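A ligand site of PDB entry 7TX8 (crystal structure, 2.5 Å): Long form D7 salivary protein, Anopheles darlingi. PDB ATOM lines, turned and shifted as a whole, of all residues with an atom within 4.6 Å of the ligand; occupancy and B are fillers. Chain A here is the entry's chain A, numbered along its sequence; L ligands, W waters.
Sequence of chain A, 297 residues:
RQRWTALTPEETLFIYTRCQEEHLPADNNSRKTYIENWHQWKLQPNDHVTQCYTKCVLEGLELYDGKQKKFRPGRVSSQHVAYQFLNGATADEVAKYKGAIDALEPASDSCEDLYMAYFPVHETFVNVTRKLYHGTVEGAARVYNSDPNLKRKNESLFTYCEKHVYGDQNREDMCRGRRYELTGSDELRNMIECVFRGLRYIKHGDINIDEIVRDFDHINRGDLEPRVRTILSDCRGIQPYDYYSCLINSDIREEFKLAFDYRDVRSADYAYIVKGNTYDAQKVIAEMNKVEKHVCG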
ATOM      1  N   LEU A  13       6.853  -3.845  17.796  1.00  0.00           N
ATOM      2  CA  LEU A  13       6.892  -5.230  18.240  1.00  0.00           C
ATOM      3  C   LEU A  13       6.902  -6.157  17.026  1.00  0.00           C
ATOM      4  O   LEU A  13       7.575  -7.197  17.015  1.00  0.00           O
ATOM      5  CB  LEU A  13       5.698  -5.529  19.128  1.00  0.00           C
ATOM      6  CG  LEU A  13       5.601  -6.918  19.762  1.00  0.00           C
ATOM      7  CD1 LEU A  13       6.809  -7.234  20.621  1.00  0.00           C
ATOM      8  CD2 LEU A  13       4.345  -7.025  20.602  1.00  0.00           C
ATOM      9  N   TYR A  16      10.555  -6.022  15.811  1.00  0.00           N
ATOM     10  CA  TYR A  16      11.505  -6.761  16.634  1.00  0.00           C
ATOM     11  C   TYR A  16      11.325  -8.254  16.472  1.00  0.00           C
ATOM     12  O   TYR A  16      12.296  -9.009  16.306  1.00  0.00           O
ATOM     13  CB  TYR A  16      11.331  -6.372  18.099  1.00  0.00           C
ATOM     14  CG  TYR A  16      11.527  -4.907  18.426  1.00  0.00           C
ATOM     15  CD1 TYR A  16      12.520  -4.145  17.780  1.00  0.00           C
ATOM     16  CD2 TYR A  16      10.723  -4.283  19.372  1.00  0.00           C
ATOM     17  CE1 TYR A  16      12.699  -2.776  18.071  1.00  0.00           C
ATOM     18  CE2 TYR A  16      10.903  -2.932  19.699  1.00  0.00           C
ATOM     19  CZ  TYR A  16      11.886  -2.182  19.035  1.00  0.00           C
ATOM     20  OH  TYR A  16      12.026  -0.843  19.357  1.00  0.00           O
ATOM     21  N   THR A  17      10.067  -8.726  16.586  1.00  0.00           N
ATOM     22  CA  THR A  17       9.841 -10.154  16.445  1.00  0.00           C
ATOM     23  C   THR A  17      10.169 -10.624  15.026  1.00  0.00           C
ATOM     24  O   THR A  17      10.805 -11.667  14.859  1.00  0.00           O
ATOM     25  CB  THR A  17       8.411 -10.537  16.851  1.00  0.00           C
ATOM     26  OG1 THR A  17       7.435  -9.813  16.088  1.00  0.00           O
ATOM     27  CG2 THR A  17       8.172 -10.271  18.312  1.00  0.00           C
ATOM     28  N   GLN A  20      13.985 -10.919  14.701  1.00  0.00           N
ATOM     29  CA  GLN A  20      14.507 -12.073  15.406  1.00  0.00           C
ATOM     30  C   GLN A  20      14.219 -13.361  14.633  1.00  0.00           C
ATOM     31  O   GLN A  20      15.106 -14.194  14.441  1.00  0.00           O
ATOM     32  CB  GLN A  20      13.932 -12.121  16.819  1.00  0.00           C
ATOM     33  CG  GLN A  20      14.421 -10.987  17.736  1.00  0.00           C
ATOM     34  CD  GLN A  20      14.497 -11.392  19.207  1.00  0.00           C
ATOM     35  OE1 GLN A  20      14.155 -12.509  19.578  1.00  0.00           O
ATOM     36  NE2 GLN A  20      14.952 -10.472  20.041  1.00  0.00           N
ATOM     37  N   TRP A  38      20.035 -10.338  22.913  1.00  0.00           N
ATOM     38  CA  TRP A  38      19.203  -9.349  22.233  1.00  0.00           C
ATOM     39  C   TRP A  38      18.047  -8.904  23.097  1.00  0.00           C
ATOM     40  O   TRP A  38      17.595  -7.754  22.990  1.00  0.00           O
ATOM     41  CB  TRP A  38      18.683  -9.896  20.903  1.00  0.00           C
ATOM     42  CG  TRP A  38      19.746 -10.170  19.891  1.00  0.00           C
ATOM     43  CD1 TRP A  38      21.056  -9.815  19.986  1.00  0.00           C
ATOM     44  CD2 TRP A  38      19.604 -10.862  18.640  1.00  0.00           C
ATOM     45  NE1 TRP A  38      21.740 -10.243  18.872  1.00  0.00           N
ATOM     46  CE2 TRP A  38      20.868 -10.882  18.027  1.00  0.00           C
ATOM     47  CE3 TRP A  38      18.533 -11.475  17.990  1.00  0.00           C
ATOM     48  CZ2 TRP A  38      21.097 -11.491  16.776  1.00  0.00           C
ATOM     49  CZ3 TRP A  38      18.753 -12.080  16.741  1.00  0.00           C
ATOM     50  CH2 TRP A  38      20.021 -12.076  16.151  1.00  0.00           C
ATOM     51  N   HIS A  39      17.551  -9.788  23.953  1.00  0.00           N
ATOM     52  CA  HIS A  39      16.472  -9.387  24.849  1.00  0.00           C
ATOM     53  C   HIS A  39      16.898  -8.238  25.752  1.00  0.00           C
ATOM     54  O   HIS A  39      16.156  -7.271  25.940  1.00  0.00           O
ATOM     55  CB  HIS A  39      16.011 -10.580  25.664  1.00  0.00           C
ATOM     56  CG  HIS A  39      14.759 -10.328  26.423  1.00  0.00           C
ATOM     57  ND1 HIS A  39      14.749  -9.948  27.747  1.00  0.00           N
ATOM     58  CD2 HIS A  39      13.454 -10.411  26.038  1.00  0.00           C
ATOM     59  CE1 HIS A  39      13.503  -9.802  28.154  1.00  0.00           C
ATOM     60  NE2 HIS A  39      12.691 -10.083  27.139  1.00  0.00           N
ATOM     61  N   TRP A  41      18.896  -6.104  24.870  1.00  0.00           N
ATOM     62  CA  TRP A  41      19.371  -5.043  23.979  1.00  0.00           C
ATOM     63  C   TRP A  41      20.908  -4.986  23.924  1.00  0.00           C
ATOM     64  O   TRP A  41      21.512  -3.942  23.669  1.00  0.00           O
ATOM     65  CB  TRP A  41      18.778  -3.698  24.395  1.00  0.00           C
ATOM     66  CG  TRP A  41      17.271  -3.615  24.073  1.00  0.00           C
ATOM     67  CD1 TRP A  41      16.255  -4.393  24.601  1.00  0.00           C
ATOM     68  CD2 TRP A  41      16.643  -2.720  23.154  1.00  0.00           C
ATOM     69  NE1 TRP A  41      15.054  -4.023  24.058  1.00  0.00           N
ATOM     70  CE2 TRP A  41      15.252  -2.995  23.188  1.00  0.00           C
ATOM     71  CE3 TRP A  41      17.102  -1.698  22.311  1.00  0.00           C
ATOM     72  CZ2 TRP A  41      14.335  -2.306  22.407  1.00  0.00           C
ATOM     73  CZ3 TRP A  41      16.184  -1.013  21.538  1.00  0.00           C
ATOM     74  CH2 TRP A  41      14.817  -1.326  21.599  1.00  0.00           C
ATOM     75  N   LEU A  43      23.937  -5.888  21.798  1.00  0.00           N
ATOM     76  CA  LEU A  43      24.272  -6.233  20.419  1.00  0.00           C
ATOM     77  C   LEU A  43      25.528  -7.092  20.375  1.00  0.00           C
ATOM     78  O   LEU A  43      26.509  -6.763  19.717  1.00  0.00           O
ATOM     79  CB  LEU A  43      24.449  -4.978  19.562  1.00  0.00           C
ATOM     80  CG  LEU A  43      23.174  -4.143  19.471  1.00  0.00           C
ATOM     81  CD1 LEU A  43      23.317  -2.979  18.537  1.00  0.00           C
ATOM     82  CD2 LEU A  43      21.957  -4.992  19.065  1.00  0.00           C
ATOM     83  N   TYR A  53      21.003  -8.784  12.214  1.00  0.00           N
ATOM     84  CA  TYR A  53      19.871  -8.460  13.073  1.00  0.00           C
ATOM     85  C   TYR A  53      19.811  -6.963  13.342  1.00  0.00           C
ATOM     86  O   TYR A  53      18.719  -6.366  13.332  1.00  0.00           O
ATOM     87  CB  TYR A  53      19.973  -9.234  14.385  1.00  0.00           C
ATOM     88  CG  TYR A  53      18.936  -8.842  15.432  1.00  0.00           C
ATOM     89  CD1 TYR A  53      17.583  -9.146  15.251  1.00  0.00           C
ATOM     90  CD2 TYR A  53      19.323  -8.185  16.606  1.00  0.00           C
ATOM     91  CE1 TYR A  53      16.649  -8.807  16.215  1.00  0.00           C
ATOM     92  CE2 TYR A  53      18.402  -7.842  17.572  1.00  0.00           C
ATOM     93  CZ  TYR A  53      17.063  -8.157  17.374  1.00  0.00           C
ATOM     94  OH  TYR A  53      16.128  -7.809  18.320  1.00  0.00           O
ATOM     95  N   VAL A  57      16.699  -4.419  12.465  1.00  0.00           N
ATOM     96  CA  VAL A  57      15.976  -3.582  13.413  1.00  0.00           C
ATOM     97  C   VAL A  57      16.079  -2.120  13.005  1.00  0.00           C
ATOM     98  O   VAL A  57      15.088  -1.381  12.974  1.00  0.00           O
ATOM     99  CB  VAL A  57      16.491  -3.823  14.846  1.00  0.00           C
ATOM    100  CG1 VAL A  57      15.847  -2.841  15.764  1.00  0.00           C
ATOM    101  CG2 VAL A  57      16.237  -5.283  15.314  1.00  0.00           C
ATOM    102  N   LEU A  58      17.281  -1.672  12.646  1.00  0.00           N
ATOM    103  CA  LEU A  58      17.466  -0.275  12.282  1.00  0.00           C
ATOM    104  C   LEU A  58      16.553   0.114  11.119  1.00  0.00           C
ATOM    105  O   LEU A  58      16.052   1.228  11.063  1.00  0.00           O
ATOM    106  CB  LEU A  58      18.925  -0.023  11.912  1.00  0.00           C
ATOM    107  CG  LEU A  58      19.986   0.129  12.992  1.00  0.00           C
ATOM    108  CD1 LEU A  58      21.342   0.173  12.321  1.00  0.00           C
ATOM    109  CD2 LEU A  58      19.769   1.400  13.778  1.00  0.00           C
ATOM    110  N   TYR A 118      26.674   2.369  13.761  1.00  0.00           N
ATOM    111  CA  TYR A 118      25.655   2.690  14.729  1.00  0.00           C
ATOM    112  C   TYR A 118      25.986   2.154  16.109  1.00  0.00           C
ATOM    113  O   TYR A 118      25.350   2.592  17.071  1.00  0.00           O
ATOM    114  CB  TYR A 118      24.294   2.147  14.286  1.00  0.00           C
ATOM    115  CG  TYR A 118      23.127   2.455  15.216  1.00  0.00           C
ATOM    116  CD1 TYR A 118      22.527   3.723  15.260  1.00  0.00           C
ATOM    117  CD2 TYR A 118      22.605   1.469  16.056  1.00  0.00           C
ATOM    118  CE1 TYR A 118      21.450   3.990  16.124  1.00  0.00           C
ATOM    119  CE2 TYR A 118      21.546   1.728  16.916  1.00  0.00           C
ATOM    120  CZ  TYR A 118      20.973   2.989  16.945  1.00  0.00           C
ATOM    121  OH  TYR A 118      19.918   3.236  17.798  1.00  0.00           O
ATOM    122  N   HIS A 122      24.360   3.102  19.792  1.00  0.00           N
ATOM    123  CA  HIS A 122      23.478   2.212  20.529  1.00  0.00           C
ATOM    124  C   HIS A 122      23.984   2.029  21.957  1.00  0.00           C
ATOM    125  O   HIS A 122      23.210   2.101  22.909  1.00  0.00           O
ATOM    126  CB  HIS A 122      23.325   0.872  19.817  1.00  0.00           C
ATOM    127  CG  HIS A 122      22.585  -0.161  20.615  1.00  0.00           C
ATOM    128  ND1 HIS A 122      21.200  -0.209  20.684  1.00  0.00           N
ATOM    129  CD2 HIS A 122      23.033  -1.184  21.386  1.00  0.00           C
ATOM    130  CE1 HIS A 122      20.834  -1.211  21.457  1.00  0.00           C
ATOM    131  NE2 HIS A 122      21.921  -1.816  21.898  1.00  0.00           N
ATOM    132  N   HIS A 134       9.273   2.353  22.104  1.00  0.00           N
ATOM    133  CA  HIS A 134       8.522   1.406  22.889  1.00  0.00           C
ATOM    134  C   HIS A 134       9.322   0.132  23.095  1.00  0.00           C
ATOM    135  O   HIS A 134       8.823  -0.978  22.959  1.00  0.00           O
ATOM    136  CB  HIS A 134       7.196   1.073  22.203  1.00  0.00           C
ATOM    137  CG  HIS A 134       6.580   2.226  21.477  1.00  0.00           C
ATOM    138  ND1 HIS A 134       6.234   3.411  22.100  1.00  0.00           N
ATOM    139  CD2 HIS A 134       6.256   2.380  20.165  1.00  0.00           C
ATOM    140  CE1 HIS A 134       5.711   4.225  21.205  1.00  0.00           C
ATOM    141  NE2 HIS A 134       5.703   3.622  20.029  1.00  0.00           N
ATOM    142  N   GLY A 135      10.594   0.285  23.448  1.00  0.00           N
ATOM    143  CA  GLY A 135      11.371  -0.903  23.730  1.00  0.00           C
ATOM    144  C   GLY A 135      11.340  -1.426  25.157  1.00  0.00           C
ATOM    145  O   GLY A 135      12.215  -2.218  25.509  1.00  0.00           O
ATOM    146  N   THR A 136      10.395  -1.021  25.997  1.00  0.00           N
ATOM    147  CA  THR A 136      10.208  -1.676  27.283  1.00  0.00           C
ATOM    148  C   THR A 136       8.758  -2.079  27.446  1.00  0.00           C
ATOM    149  O   THR A 136       7.852  -1.439  26.907  1.00  0.00           O
ATOM    150  CB  THR A 136      10.561  -0.790  28.459  1.00  0.00           C
ATOM    151  OG1 THR A 136       9.553   0.213  28.536  1.00  0.00           O
ATOM    152  CG2 THR A 136      12.008  -0.184  28.341  1.00  0.00           C
ATOM    153  N   VAL A 137       8.536  -3.125  28.250  1.00  0.00           N
ATOM    154  CA  VAL A 137       7.191  -3.596  28.511  1.00  0.00           C
ATOM    155  C   VAL A 137       6.373  -2.532  29.250  1.00  0.00           C
ATOM    156  O   VAL A 137       5.190  -2.330  28.958  1.00  0.00           O
ATOM    157  CB  VAL A 137       7.260  -4.930  29.280  1.00  0.00           C
ATOM    158  CG1 VAL A 137       8.123  -4.722  30.415  1.00  0.00           C
ATOM    159  CG2 VAL A 137       5.916  -5.329  29.800  1.00  0.00           C
ATOM    160  N   ALA A 140       5.662   0.510  26.457  1.00  0.00           N
ATOM    161  CA  ALA A 140       4.672  -0.026  25.531  1.00  0.00           C
ATOM    162  C   ALA A 140       3.317  -0.198  26.207  1.00  0.00           C
ATOM    163  O   ALA A 140       2.282   0.095  25.611  1.00  0.00           O
ATOM    164  CB  ALA A 140       5.115  -1.354  24.915  1.00  0.00           C
ATOM    165  N   LYS A 153      -0.936  -7.168  22.589  1.00  0.00           N
ATOM    166  CA  LYS A 153       0.027  -8.255  22.427  1.00  0.00           C
ATOM    167  C   LYS A 153      -0.658  -9.584  22.187  1.00  0.00           C
ATOM    168  O   LYS A 153      -0.376 -10.292  21.210  1.00  0.00           O
ATOM    169  CB  LYS A 153       0.918  -8.369  23.659  1.00  0.00           C
ATOM    170  CG  LYS A 153       1.896  -7.242  23.861  1.00  0.00           C
ATOM    171  CD  LYS A 153       2.259  -7.120  25.352  1.00  0.00           C
ATOM    172  CE  LYS A 153       2.689  -8.459  25.956  1.00  0.00           C
ATOM    173  NZ  LYS A 153       2.974  -8.288  27.406  1.00  0.00           N
HETATM  174  C1  LIG L   1       5.895  -6.631  25.092  1.00  0.00           C
HETATM  175  O1  LIG L   1       5.931  -7.674  25.804  1.00  0.00           O
HETATM  176  C2  LIG L   1       7.223  -6.146  24.537  1.00  0.00           C
HETATM  177  O2  LIG L   1       4.848  -5.987  24.803  1.00  0.00           O
HETATM  178  C3  LIG L   1       7.447  -4.645  24.580  1.00  0.00           C
HETATM  179  O3  LIG L   1      17.068  -6.415  20.805  1.00  0.00           O
HETATM  180  C4  LIG L   1       8.731  -4.245  23.895  1.00  0.00           C
HETATM  181  C5  LIG L   1       9.925  -4.532  24.736  1.00  0.00           C
HETATM  182  O4  LIG L   1      11.105  -8.545  21.092  1.00  0.00           O
HETATM  183  C6  LIG L   1      11.102  -4.919  24.290  1.00  0.00           C
HETATM  184  C7  LIG L   1      11.454  -5.205  22.873  1.00  0.00           C
HETATM  185  C8  LIG L   1      12.322  -6.448  22.781  1.00  0.00           C
HETATM  186  C9  LIG L   1      11.586  -7.714  23.264  1.00  0.00           C
HETATM  187  C10 LIG L   1      12.573  -8.800  22.868  1.00  0.00           C
HETATM  188  C11 LIG L   1      12.511  -8.392  21.398  1.00  0.00           C
HETATM  189  C12 LIG L   1      12.815  -6.892  21.405  1.00  0.00           C
HETATM  190  C13 LIG L   1      14.285  -6.628  21.252  1.00  0.00           C
HETATM  191  C14 LIG L   1      14.809  -5.551  20.736  1.00  0.00           C
HETATM  192  C15 LIG L   1      16.275  -5.239  20.618  1.00  0.00           C
HETATM  193  C16 LIG L   1      16.650  -4.657  19.270  1.00  0.00           C
HETATM  194  C17 LIG L   1      18.072  -4.147  19.172  1.00  0.00           C
HETATM  195  C18 LIG L   1      18.104  -2.697  18.770  1.00  0.00           C
HETATM  196  C19 LIG L   1      18.940  -2.363  17.570  1.00  0.00           C
HETATM  197  C20 LIG L   1      18.852  -0.927  17.152  1.00  0.00           C
HETATM  198  C21 LIG L   1      10.452  -7.981  22.273  1.00  0.00           C
HETATM  199  O   HOH W   1       4.726  -4.248  22.462  1.00  0.00           O
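O1 of the ligand lies within salt-bridge range of NZ of Lys 153 (3.4 Å). The side-chain hydroxyl of Tyr 53 lies within hydrogen-bond range of an oxygen (O3) of the ligand (3.0 Å). O of Trp 38 lies within hydrogen-bond range of O3 of the ligand, 2.6 Å away.
The backbone carbonyl oxygen of Trp 41 sits at hydrogen-bond distance from a ring nitrogen (NE2) of His 122. The side-chain hydroxyl of Tyr 53 is in hydrogen-bond range of the side-chain amide nitrogen of Gln 20 (3.4 Å).
Residues that only touch the ligand: Gly 135, His 134, Gln 20, Trp 41, Val 57, Tyr 16, His 39, Thr 136, Tyr 118 and Leu 43. Hydrophobic or aromatic side chains that line the ligand: Tyr 16, Trp 38, His 39, Trp 41, Leu 43, Tyr 53, Val 57 and Tyr 118.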
